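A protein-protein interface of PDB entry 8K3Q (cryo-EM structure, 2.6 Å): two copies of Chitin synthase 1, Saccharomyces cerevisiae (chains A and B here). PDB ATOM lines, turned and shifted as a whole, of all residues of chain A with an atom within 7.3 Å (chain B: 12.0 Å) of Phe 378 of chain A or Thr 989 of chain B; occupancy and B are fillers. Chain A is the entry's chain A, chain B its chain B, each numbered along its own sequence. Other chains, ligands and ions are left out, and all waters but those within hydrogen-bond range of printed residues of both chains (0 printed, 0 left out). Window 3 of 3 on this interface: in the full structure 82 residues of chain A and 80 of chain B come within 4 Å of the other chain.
N of Phe 378 of chain A lies within hydrogen-bond range of O of Phe 990 of chain B (3.0 Å). N of Leu 380 of chain A sits at hydrogen-bond distance from O of Gly 988 of chain B (3.1 Å).
The backbone NH of Leu 255 of chain A lies within hydrogen-bond range of the backbone carbonyl oxygen of Lys 377 of chain A (2.8 Å).
Ile 375 of chain A touches Lys 991 of chain B (CG2 to CB, 3.6 Å). Ile 375 of chain A touches Met 992 of chain B (CA to O, 3.2 Å). O of Arg 376 of chain A touches O of Phe 990 of chain B, at 3.6 Å. Arg 376 of chain A touches Lys 991 of chain B (O to CA, 3.4 Å). O of Arg 376 of chain A touches N of Met 992 of chain B (3.7 Å). Lys 377 of chain A touches Phe 990 of chain B. CE2 of Phe 378 of chain A touches CB of Met 992 of chain B (3.5 Å). CA of Lys 379 of chain A touches O of Gly 988 of chain B (3.4 Å). Leu 380 of chain A touches Phe 990 of chain B. Phe 385 of chain A touches Phe 990 of chain B.
No residue of chain B comes within 4 Å of Ser 253 of chain A. No residue of chain B comes within 4 Å of Tyr 254 of chain A. No residue of chain B comes within 4 Å of Leu 255 of chain A. Of the printed residues of chain B, Ile 375 of chain A touches Lys 991 (3.6 Å) and Met 992 (3.2 Å). Of the printed residues of chain B, Arg 376 of chain A touches Phe 990, Lys 991 and Met 992. Lys 377 of chain A touches just one residue of chain B: Phe 990. Phe 378 of chain A touches just these residues of chain B: Thr 989, Phe 990 and Met 992. Of the printed residues of chain B, Phe 385 of chain A touches Phe 990. Of chain A, only Lys 379 and Leu 380 come within 4 Å of Gly 988 of chain B. Thr 989 of chain B touches one residue of chain A. Printed residues of chain A within 4 Å of Phe 990 of chain B: Arg 376 (3.6 Å), Lys 377 (3.6 Å), Phe 378 (3.0 Å), Leu 380 (3.9 Å) and Phe 385 (3.99 Å). Of the printed residues of chain A, Lys 991 of chain B touches Ile 375 (3.6 Å) and Arg 376 (3.4 Å). The nearest printed residue of chain A that does not touch Met 992 of chain B is Phe 385 of chain A (4.3 Å).
Printed residues of chain B that touch a printed residue of chain A: Gly 988, Thr 989, Phe 990, Lys 991 and Met 992. Hydrophobic or aromatic side chains of chain B within 4 Å of the printed part of chain A: Phe 990 and Met 992. Printed residues of chain A that touch a printed residue of chain B: Ile 375, Arg 376, Lys 377, Phe 378, Lys 379, Leu 380 and Phe 385. Hydrophobic or aromatic side chains of chain A that line the printed part of chain B: Ile 375, Phe 378 and Phe 385. Among the printed residues, 13 pairs touch across the chains. Among the printed residues, no Asp or Glu carboxylate lies within 4 Å of a Lys or Arg side-chain nitrogen of the other chain.
No position is printed for both chains. Of the 13 pairs that touch across the chains among the printed residues, none has its exchanged pair printed and touching as well.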
ATOM      1  N   ASN A 252      11.081   0.435 -14.187  1.00  0.00           N
ATOM      2  CA  ASN A 252      11.866   0.909 -13.055  1.00  0.00           C
ATOM      3  C   ASN A 252      10.949   1.738 -12.162  1.00  0.00           C
ATOM      4  O   ASN A 252      10.903   2.964 -12.288  1.00  0.00           O
ATOM      5  CB  ASN A 252      13.049   1.741 -13.544  1.00  0.00           C
ATOM      6  CG  ASN A 252      14.246   1.651 -12.626  1.00  0.00           C
ATOM      7  OD1 ASN A 252      14.777   0.571 -12.388  1.00  0.00           O
ATOM      8  ND2 ASN A 252      14.677   2.790 -12.102  1.00  0.00           N
ATOM      9  N   SER A 253      10.202   1.075 -11.268  1.00  0.00           N
ATOM     10  CA  SER A 253       9.231   1.783 -10.450  1.00  0.00           C
ATOM     11  C   SER A 253       9.841   2.100  -9.088  1.00  0.00           C
ATOM     12  O   SER A 253      10.175   3.268  -8.829  1.00  0.00           O
ATOM     13  CB  SER A 253       7.944   0.958 -10.343  1.00  0.00           C
ATOM     14  OG  SER A 253       8.245  -0.398 -10.063  1.00  0.00           O
ATOM     15  N   TYR A 254      10.059   1.112  -8.223  1.00  0.00           N
ATOM     16  CA  TYR A 254      10.597   1.318  -6.881  1.00  0.00           C
ATOM     17  C   TYR A 254      10.652  -0.019  -6.160  1.00  0.00           C
ATOM     18  O   TYR A 254      10.099  -1.020  -6.623  1.00  0.00           O
ATOM     19  CB  TYR A 254       9.798   2.343  -6.057  1.00  0.00           C
ATOM     20  CG  TYR A 254       8.339   2.025  -5.816  1.00  0.00           C
ATOM     21  CD1 TYR A 254       7.360   2.489  -6.679  1.00  0.00           C
ATOM     22  CD2 TYR A 254       7.940   1.266  -4.730  1.00  0.00           C
ATOM     23  CE1 TYR A 254       6.028   2.213  -6.464  1.00  0.00           C
ATOM     24  CE2 TYR A 254       6.609   0.978  -4.512  1.00  0.00           C
ATOM     25  CZ  TYR A 254       5.658   1.455  -5.383  1.00  0.00           C
ATOM     26  OH  TYR A 254       4.328   1.177  -5.175  1.00  0.00           O
ATOM     27  N   LEU A 255      11.310  -0.013  -5.007  1.00  0.00           N
ATOM     28  CA  LEU A 255      11.626  -1.230  -4.276  1.00  0.00           C
ATOM     29  C   LEU A 255      10.724  -1.370  -3.059  1.00  0.00           C
ATOM     30  O   LEU A 255      10.441  -0.388  -2.366  1.00  0.00           O
ATOM     31  CB  LEU A 255      13.092  -1.226  -3.843  1.00  0.00           C
ATOM     32  CG  LEU A 255      14.085  -1.281  -5.006  1.00  0.00           C
ATOM     33  CD1 LEU A 255      15.514  -1.133  -4.519  1.00  0.00           C
ATOM     34  CD2 LEU A 255      13.912  -2.563  -5.794  1.00  0.00           C
ATOM     35  N   GLY A 256      10.278  -2.596  -2.801  1.00  0.00           N
ATOM     36  CA  GLY A 256       9.382  -2.855  -1.690  1.00  0.00           C
ATOM     37  C   GLY A 256      10.064  -3.362  -0.435  1.00  0.00           C
ATOM     38  O   GLY A 256      11.136  -2.878  -0.056  1.00  0.00           O
ATOM     39  N   MET A 261      12.393  -5.432  -7.142  1.00  0.00           N
ATOM     40  CA  MET A 261      11.493  -4.456  -7.745  1.00  0.00           C
ATOM     41  C   MET A 261      10.156  -5.066  -8.131  1.00  0.00           C
ATOM     42  O   MET A 261      10.097  -6.195  -8.627  1.00  0.00           O
ATOM     43  CB  MET A 261      12.160  -3.819  -8.961  1.00  0.00           C
ATOM     44  CG  MET A 261      11.371  -2.707  -9.595  1.00  0.00           C
ATOM     45  SD  MET A 261      12.288  -2.050 -10.987  1.00  0.00           S
ATOM     46  CE  MET A 261      13.590  -1.197 -10.105  1.00  0.00           C
ATOM     47  N   ILE A 375       5.506   6.920   1.164  1.00  0.00           N
ATOM     48  CA  ILE A 375       6.956   7.079   1.150  1.00  0.00           C
ATOM     49  C   ILE A 375       7.644   5.740   0.918  1.00  0.00           C
ATOM     50  O   ILE A 375       7.765   4.923   1.829  1.00  0.00           O
ATOM     51  CB  ILE A 375       7.458   7.734   2.444  1.00  0.00           C
ATOM     52  CG1 ILE A 375       6.832   9.116   2.618  1.00  0.00           C
ATOM     53  CG2 ILE A 375       8.953   7.857   2.423  1.00  0.00           C
ATOM     54  CD1 ILE A 375       7.242   9.811   3.895  1.00  0.00           C
ATOM     55  N   ARG A 376       8.107   5.533  -0.311  1.00  0.00           N
ATOM     56  CA  ARG A 376       8.664   4.264  -0.748  1.00  0.00           C
ATOM     57  C   ARG A 376      10.161   4.401  -0.992  1.00  0.00           C
ATOM     58  O   ARG A 376      10.697   5.510  -1.071  1.00  0.00           O
ATOM     59  CB  ARG A 376       7.974   3.778  -2.025  1.00  0.00           C
ATOM     60  CG  ARG A 376       6.473   4.012  -2.042  1.00  0.00           C
ATOM     61  CD  ARG A 376       5.756   3.098  -1.070  1.00  0.00           C
ATOM     62  NE  ARG A 376       5.210   1.920  -1.732  1.00  0.00           N
ATOM     63  CZ  ARG A 376       4.456   1.010  -1.126  1.00  0.00           C
ATOM     64  NH1 ARG A 376       4.161   1.142   0.158  1.00  0.00           N
ATOM     65  NH2 ARG A 376       3.998  -0.034  -1.801  1.00  0.00           N
ATOM     66  N   LYS A 377      10.832   3.260  -1.111  1.00  0.00           N
ATOM     67  CA  LYS A 377      12.272   3.229  -1.318  1.00  0.00           C
ATOM     68  C   LYS A 377      12.587   3.053  -2.797  1.00  0.00           C
ATOM     69  O   LYS A 377      12.129   2.096  -3.429  1.00  0.00           O
ATOM     70  CB  LYS A 377      12.903   2.101  -0.504  1.00  0.00           C
ATOM     71  N   PHE A 378      13.385   3.964  -3.337  1.00  0.00           N
ATOM     72  CA  PHE A 378      13.717   4.000  -4.751  1.00  0.00           C
ATOM     73  C   PHE A 378      15.183   3.627  -4.944  1.00  0.00           C
ATOM     74  O   PHE A 378      15.878   3.249  -4.002  1.00  0.00           O
ATOM     75  CB  PHE A 378      13.422   5.382  -5.336  1.00  0.00           C
ATOM     76  CG  PHE A 378      11.959   5.675  -5.486  1.00  0.00           C
ATOM     77  CD1 PHE A 378      11.360   5.633  -6.726  1.00  0.00           C
ATOM     78  CD2 PHE A 378      11.184   5.987  -4.387  1.00  0.00           C
ATOM     79  CE1 PHE A 378      10.025   5.903  -6.867  1.00  0.00           C
ATOM     80  CE2 PHE A 378       9.844   6.253  -4.525  1.00  0.00           C
ATOM     81  CZ  PHE A 378       9.265   6.210  -5.765  1.00  0.00           C
ATOM     82  N   LYS A 379      15.645   3.723  -6.188  1.00  0.00           N
ATOM     83  CA  LYS A 379      17.051   3.499  -6.507  1.00  0.00           C
ATOM     84  C   LYS A 379      17.341   4.098  -7.871  1.00  0.00           C
ATOM     85  O   LYS A 379      16.672   3.749  -8.847  1.00  0.00           O
ATOM     86  CB  LYS A 379      17.397   2.012  -6.499  1.00  0.00           C
ATOM     87  CG  LYS A 379      18.879   1.739  -6.653  1.00  0.00           C
ATOM     88  CD  LYS A 379      19.185   0.260  -6.538  1.00  0.00           C
ATOM     89  CE  LYS A 379      18.717  -0.483  -7.774  1.00  0.00           C
ATOM     90  NZ  LYS A 379      19.106  -1.917  -7.745  1.00  0.00           N
ATOM     91  N   LEU A 380      18.328   4.991  -7.939  1.00  0.00           N
ATOM     92  CA  LEU A 380      18.761   5.526  -9.222  1.00  0.00           C
ATOM     93  C   LEU A 380      19.216   4.390 -10.121  1.00  0.00           C
ATOM     94  O   LEU A 380      20.030   3.557  -9.718  1.00  0.00           O
ATOM     95  CB  LEU A 380      19.898   6.527  -9.036  1.00  0.00           C
ATOM     96  N   PHE A 385      17.643   9.377 -12.752  1.00  0.00           N
ATOM     97  CA  PHE A 385      16.292   9.110 -12.269  1.00  0.00           C
ATOM     98  C   PHE A 385      15.399   8.687 -13.425  1.00  0.00           C
ATOM     99  O   PHE A 385      15.155   9.464 -14.352  1.00  0.00           O
ATOM    100  CB  PHE A 385      15.720  10.337 -11.570  1.00  0.00           C
ATOM    101  CG  PHE A 385      14.415  10.086 -10.886  1.00  0.00           C
ATOM    102  CD1 PHE A 385      14.145   8.861 -10.312  1.00  0.00           C
ATOM    103  CD2 PHE A 385      13.450  11.071 -10.832  1.00  0.00           C
ATOM    104  CE1 PHE A 385      12.943   8.630  -9.691  1.00  0.00           C
ATOM    105  CE2 PHE A 385      12.247  10.843 -10.214  1.00  0.00           C
ATOM    106  CZ  PHE A 385      11.994   9.623  -9.643  1.00  0.00           C
ATOM    107  N   VAL A 386      14.911   7.454 -13.367  1.00  0.00           N
ATOM    108  CA  VAL A 386      13.947   6.929 -14.320  1.00  0.00           C
ATOM    109  C   VAL A 386      12.788   6.335 -13.538  1.00  0.00           C
ATOM    110  O   VAL A 386      12.986   5.421 -12.730  1.00  0.00           O
ATOM    111  CB  VAL A 386      14.591   5.876 -15.236  1.00  0.00           C
ATOM    112  CG1 VAL A 386      13.608   5.414 -16.266  1.00  0.00           C
ATOM    113  CG2 VAL A 386      15.807   6.458 -15.895  1.00  0.00           C
ATOM    114  N   PHE A 387      11.583   6.834 -13.780  1.00  0.00           N
ATOM    115  CA  PHE A 387      10.418   6.339 -13.062  1.00  0.00           C
ATOM    116  C   PHE A 387       9.331   5.924 -14.045  1.00  0.00           C
ATOM    117  O   PHE A 387       9.192   6.483 -15.130  1.00  0.00           O
ATOM    118  CB  PHE A 387       9.883   7.382 -12.076  1.00  0.00           C
ATOM    119  CG  PHE A 387       8.768   6.871 -11.212  1.00  0.00           C
ATOM    120  CD1 PHE A 387       7.555   7.520 -11.165  1.00  0.00           C
ATOM    121  CD2 PHE A 387       8.931   5.727 -10.462  1.00  0.00           C
ATOM    122  CE1 PHE A 387       6.536   7.041 -10.380  1.00  0.00           C
ATOM    123  CE2 PHE A 387       7.913   5.246  -9.677  1.00  0.00           C
ATOM    124  CZ  PHE A 387       6.719   5.903  -9.636  1.00  0.00           C
ATOM    125  N   ASP A 388       8.537   4.944 -13.625  1.00  0.00           N
ATOM    126  CA  ASP A 388       7.498   4.361 -14.465  1.00  0.00           C
ATOM    127  C   ASP A 388       6.172   4.425 -13.734  1.00  0.00           C
ATOM    128  O   ASP A 388       5.959   3.694 -12.765  1.00  0.00           O
ATOM    129  CB  ASP A 388       7.856   2.931 -14.829  1.00  0.00           C
ATOM    130  CG  ASP A 388       7.952   2.732 -16.303  1.00  0.00           C
ATOM    131  OD1 ASP A 388       7.449   3.602 -17.033  1.00  0.00           O
ATOM    132  OD2 ASP A 388       8.579   1.757 -16.745  1.00  0.00           O
ATOM    133  N   LYS B 981      13.702  18.084  -5.199  1.00  0.00           N
ATOM    134  CA  LYS B 981      15.135  17.837  -5.243  1.00  0.00           C
ATOM    135  C   LYS B 981      15.370  16.373  -4.900  1.00  0.00           C
ATOM    136  O   LYS B 981      14.544  15.741  -4.242  1.00  0.00           O
ATOM    137  CB  LYS B 981      15.877  18.736  -4.243  1.00  0.00           C
ATOM    138  N   ILE B 982      16.508  15.837  -5.337  1.00  0.00           N
ATOM    139  CA  ILE B 982      16.874  14.456  -5.032  1.00  0.00           C
ATOM    140  C   ILE B 982      18.284  14.409  -4.464  1.00  0.00           C
ATOM    141  O   ILE B 982      19.239  14.860  -5.105  1.00  0.00           O
ATOM    142  CB  ILE B 982      16.779  13.537  -6.263  1.00  0.00           C
ATOM    143  CG1 ILE B 982      15.347  13.505  -6.785  1.00  0.00           C
ATOM    144  CG2 ILE B 982      17.294  12.153  -5.917  1.00  0.00           C
ATOM    145  CD1 ILE B 982      14.775  12.114  -6.918  1.00  0.00           C
ATOM    146  N   ASN B 983      18.406  13.853  -3.263  1.00  0.00           N
ATOM    147  CA  ASN B 983      19.679  13.571  -2.617  1.00  0.00           C
ATOM    148  C   ASN B 983      19.663  12.106  -2.215  1.00  0.00           C
ATOM    149  O   ASN B 983      18.797  11.686  -1.443  1.00  0.00           O
ATOM    150  CB  ASN B 983      19.862  14.457  -1.388  1.00  0.00           C
ATOM    151  CG  ASN B 983      20.010  15.925  -1.742  1.00  0.00           C
ATOM    152  OD1 ASN B 983      20.292  16.274  -2.883  1.00  0.00           O
ATOM    153  ND2 ASN B 983      19.790  16.793  -0.764  1.00  0.00           N
ATOM    154  N   THR B 984      20.599  11.325  -2.742  1.00  0.00           N
ATOM    155  CA  THR B 984      20.538   9.884  -2.562  1.00  0.00           C
ATOM    156  C   THR B 984      21.575   9.398  -1.559  1.00  0.00           C
ATOM    157  O   THR B 984      22.595  10.047  -1.320  1.00  0.00           O
ATOM    158  CB  THR B 984      20.738   9.162  -3.892  1.00  0.00           C
ATOM    159  OG1 THR B 984      22.069   9.393  -4.367  1.00  0.00           O
ATOM    160  CG2 THR B 984      19.753   9.680  -4.911  1.00  0.00           C
ATOM    161  N   THR B 985      21.299   8.233  -0.979  1.00  0.00           N
ATOM    162  CA  THR B 985      22.215   7.606  -0.043  1.00  0.00           C
ATOM    163  C   THR B 985      23.365   6.934  -0.791  1.00  0.00           C
ATOM    164  O   THR B 985      23.550   7.103  -2.000  1.00  0.00           O
ATOM    165  CB  THR B 985      21.487   6.577   0.824  1.00  0.00           C
ATOM    166  N   GLU B 986      24.163   6.172  -0.040  1.00  0.00           N
ATOM    167  CA  GLU B 986      25.294   5.469  -0.635  1.00  0.00           C
ATOM    168  C   GLU B 986      24.838   4.411  -1.631  1.00  0.00           C
ATOM    169  O   GLU B 986      25.405   4.289  -2.724  1.00  0.00           O
ATOM    170  CB  GLU B 986      26.145   4.838   0.468  1.00  0.00           C
ATOM    171  N   ASP B 987      23.804   3.647  -1.280  1.00  0.00           N
ATOM    172  CA  ASP B 987      23.303   2.584  -2.145  1.00  0.00           C
ATOM    173  C   ASP B 987      22.595   3.114  -3.381  1.00  0.00           C
ATOM    174  O   ASP B 987      22.102   2.312  -4.183  1.00  0.00           O
ATOM    175  CB  ASP B 987      22.343   1.680  -1.368  1.00  0.00           C
ATOM    176  N   GLY B 988      22.538   4.432  -3.556  1.00  0.00           N
ATOM    177  CA  GLY B 988      21.709   5.021  -4.582  1.00  0.00           C
ATOM    178  C   GLY B 988      20.245   5.100  -4.230  1.00  0.00           C
ATOM    179  O   GLY B 988      19.435   5.438  -5.095  1.00  0.00           O
ATOM    180  N   THR B 989      19.880   4.804  -2.988  1.00  0.00           N
ATOM    181  CA  THR B 989      18.485   4.762  -2.581  1.00  0.00           C
ATOM    182  C   THR B 989      18.063   6.081  -1.950  1.00  0.00           C
ATOM    183  O   THR B 989      18.889   6.858  -1.468  1.00  0.00           O
ATOM    184  CB  THR B 989      18.228   3.622  -1.593  1.00  0.00           C
ATOM    185  N   PHE B 990      16.756   6.324  -1.966  1.00  0.00           N
ATOM    186  CA  PHE B 990      16.180   7.542  -1.427  1.00  0.00           C
ATOM    187  C   PHE B 990      14.688   7.324  -1.221  1.00  0.00           C
ATOM    188  O   PHE B 990      14.135   6.295  -1.616  1.00  0.00           O
ATOM    189  CB  PHE B 990      16.470   8.746  -2.336  1.00  0.00           C
ATOM    190  CG  PHE B 990      15.987   8.582  -3.750  1.00  0.00           C
ATOM    191  CD1 PHE B 990      16.727   7.852  -4.663  1.00  0.00           C
ATOM    192  CD2 PHE B 990      14.802   9.157  -4.169  1.00  0.00           C
ATOM    193  CE1 PHE B 990      16.296   7.700  -5.961  1.00  0.00           C
ATOM    194  CE2 PHE B 990      14.365   9.001  -5.466  1.00  0.00           C
ATOM    195  CZ  PHE B 990      15.113   8.276  -6.362  1.00  0.00           C
ATOM    196  N   LYS B 991      14.044   8.289  -0.573  1.00  0.00           N
ATOM    197  CA  LYS B 991      12.620   8.216  -0.277  1.00  0.00           C
ATOM    198  C   LYS B 991      11.887   9.390  -0.909  1.00  0.00           C
ATOM    199  O   LYS B 991      12.469  10.463  -1.102  1.00  0.00           O
ATOM    200  CB  LYS B 991      12.375   8.178   1.232  1.00  0.00           C
ATOM    201  N   MET B 992      10.613   9.179  -1.233  1.00  0.00           N
ATOM    202  CA  MET B 992       9.862  10.100  -2.074  1.00  0.00           C
ATOM    203  C   MET B 992       8.416  10.175  -1.616  1.00  0.00           C
ATOM    204  O   MET B 992       7.927   9.276  -0.930  1.00  0.00           O
ATOM    205  CB  MET B 992       9.899   9.647  -3.538  1.00  0.00           C
ATOM    206  CG  MET B 992      11.268   9.703  -4.164  1.00  0.00           C
ATOM    207  SD  MET B 992      11.884  11.376  -4.290  1.00  0.00           S
ATOM    208  CE  MET B 992      11.288  11.751  -5.925  1.00  0.00           C
ATOM    209  N   GLU B 993       7.739  11.252  -1.997  1.00  0.00           N
ATOM    210  CA  GLU B 993       6.287  11.303  -1.897  1.00  0.00           C
ATOM    211  C   GLU B 993       5.686  11.150  -3.290  1.00  0.00           C
ATOM    212  O   GLU B 993       5.759  12.072  -4.111  1.00  0.00           O
ATOM    213  CB  GLU B 993       5.845  12.617  -1.260  1.00  0.00           C
ATOM    214  N   VAL B 994       5.084   9.995  -3.561  1.00  0.00           N
ATOM    215  CA  VAL B 994       4.603   9.669  -4.895  1.00  0.00           C
ATOM    216  C   VAL B 994       3.110   9.384  -4.844  1.00  0.00           C
ATOM    217  O   VAL B 994       2.611   8.752  -3.908  1.00  0.00           O
ATOM    218  CB  VAL B 994       5.360   8.463  -5.490  1.00  0.00           C
ATOM    219  N   LEU B 995       2.391   9.867  -5.856  1.00  0.00           N
ATOM    220  CA  LEU B 995       0.998   9.479  -6.038  1.00  0.00           C
ATOM    221  C   LEU B 995       0.955   7.996  -6.367  1.00  0.00           C
ATOM    222  O   LEU B 995       1.292   7.589  -7.484  1.00  0.00           O
ATOM    223  CB  LEU B 995       0.345  10.299  -7.146  1.00  0.00           C
ATOM    224  N   VAL B 996       0.551   7.182  -5.398  1.00  0.00           N
ATOM    225  CA  VAL B 996       0.527   5.739  -5.563  1.00  0.00           C
ATOM    226  C   VAL B 996      -0.885   5.227  -5.798  1.00  0.00           C
ATOM    227  O   VAL B 996      -1.102   4.374  -6.659  1.00  0.00           O
ATOM    228  CB  VAL B 996       1.170   5.051  -4.342  1.00  0.00           C
ATOM    229  N   SER B 997      -1.850   5.738  -5.041  1.00  0.00           N
ATOM    230  CA  SER B 997      -3.222   5.277  -5.177  1.00  0.00           C
ATOM    231  C   SER B 997      -3.753   5.586  -6.569  1.00  0.00           C
ATOM    232  O   SER B 997      -3.517   6.665  -7.117  1.00  0.00           O
ATOM    233  CB  SER B 997      -4.107   5.936  -4.120  1.00  0.00           C
ATOM    234  OG  SER B 997      -4.289   7.310  -4.405  1.00  0.00           O
ATOM    235  N   ILE B1001      -4.200   9.345  -9.200  1.00  0.00           N
ATOM    236  CA  ILE B1001      -3.840   9.431 -10.613  1.00  0.00           C
ATOM    237  C   ILE B1001      -5.065   9.767 -11.446  1.00  0.00           C
ATOM    238  O   ILE B1001      -5.020  10.631 -12.331  1.00  0.00           O
ATOM    239  CB  ILE B1001      -3.179   8.119 -11.074  1.00  0.00           C
ATOM    240  CG1 ILE B1001      -1.866   7.900 -10.322  1.00  0.00           C
ATOM    241  CG2 ILE B1001      -2.942   8.142 -12.569  1.00  0.00           C
ATOM    242  CD1 ILE B1001      -1.270   6.533 -10.524  1.00  0.00           C
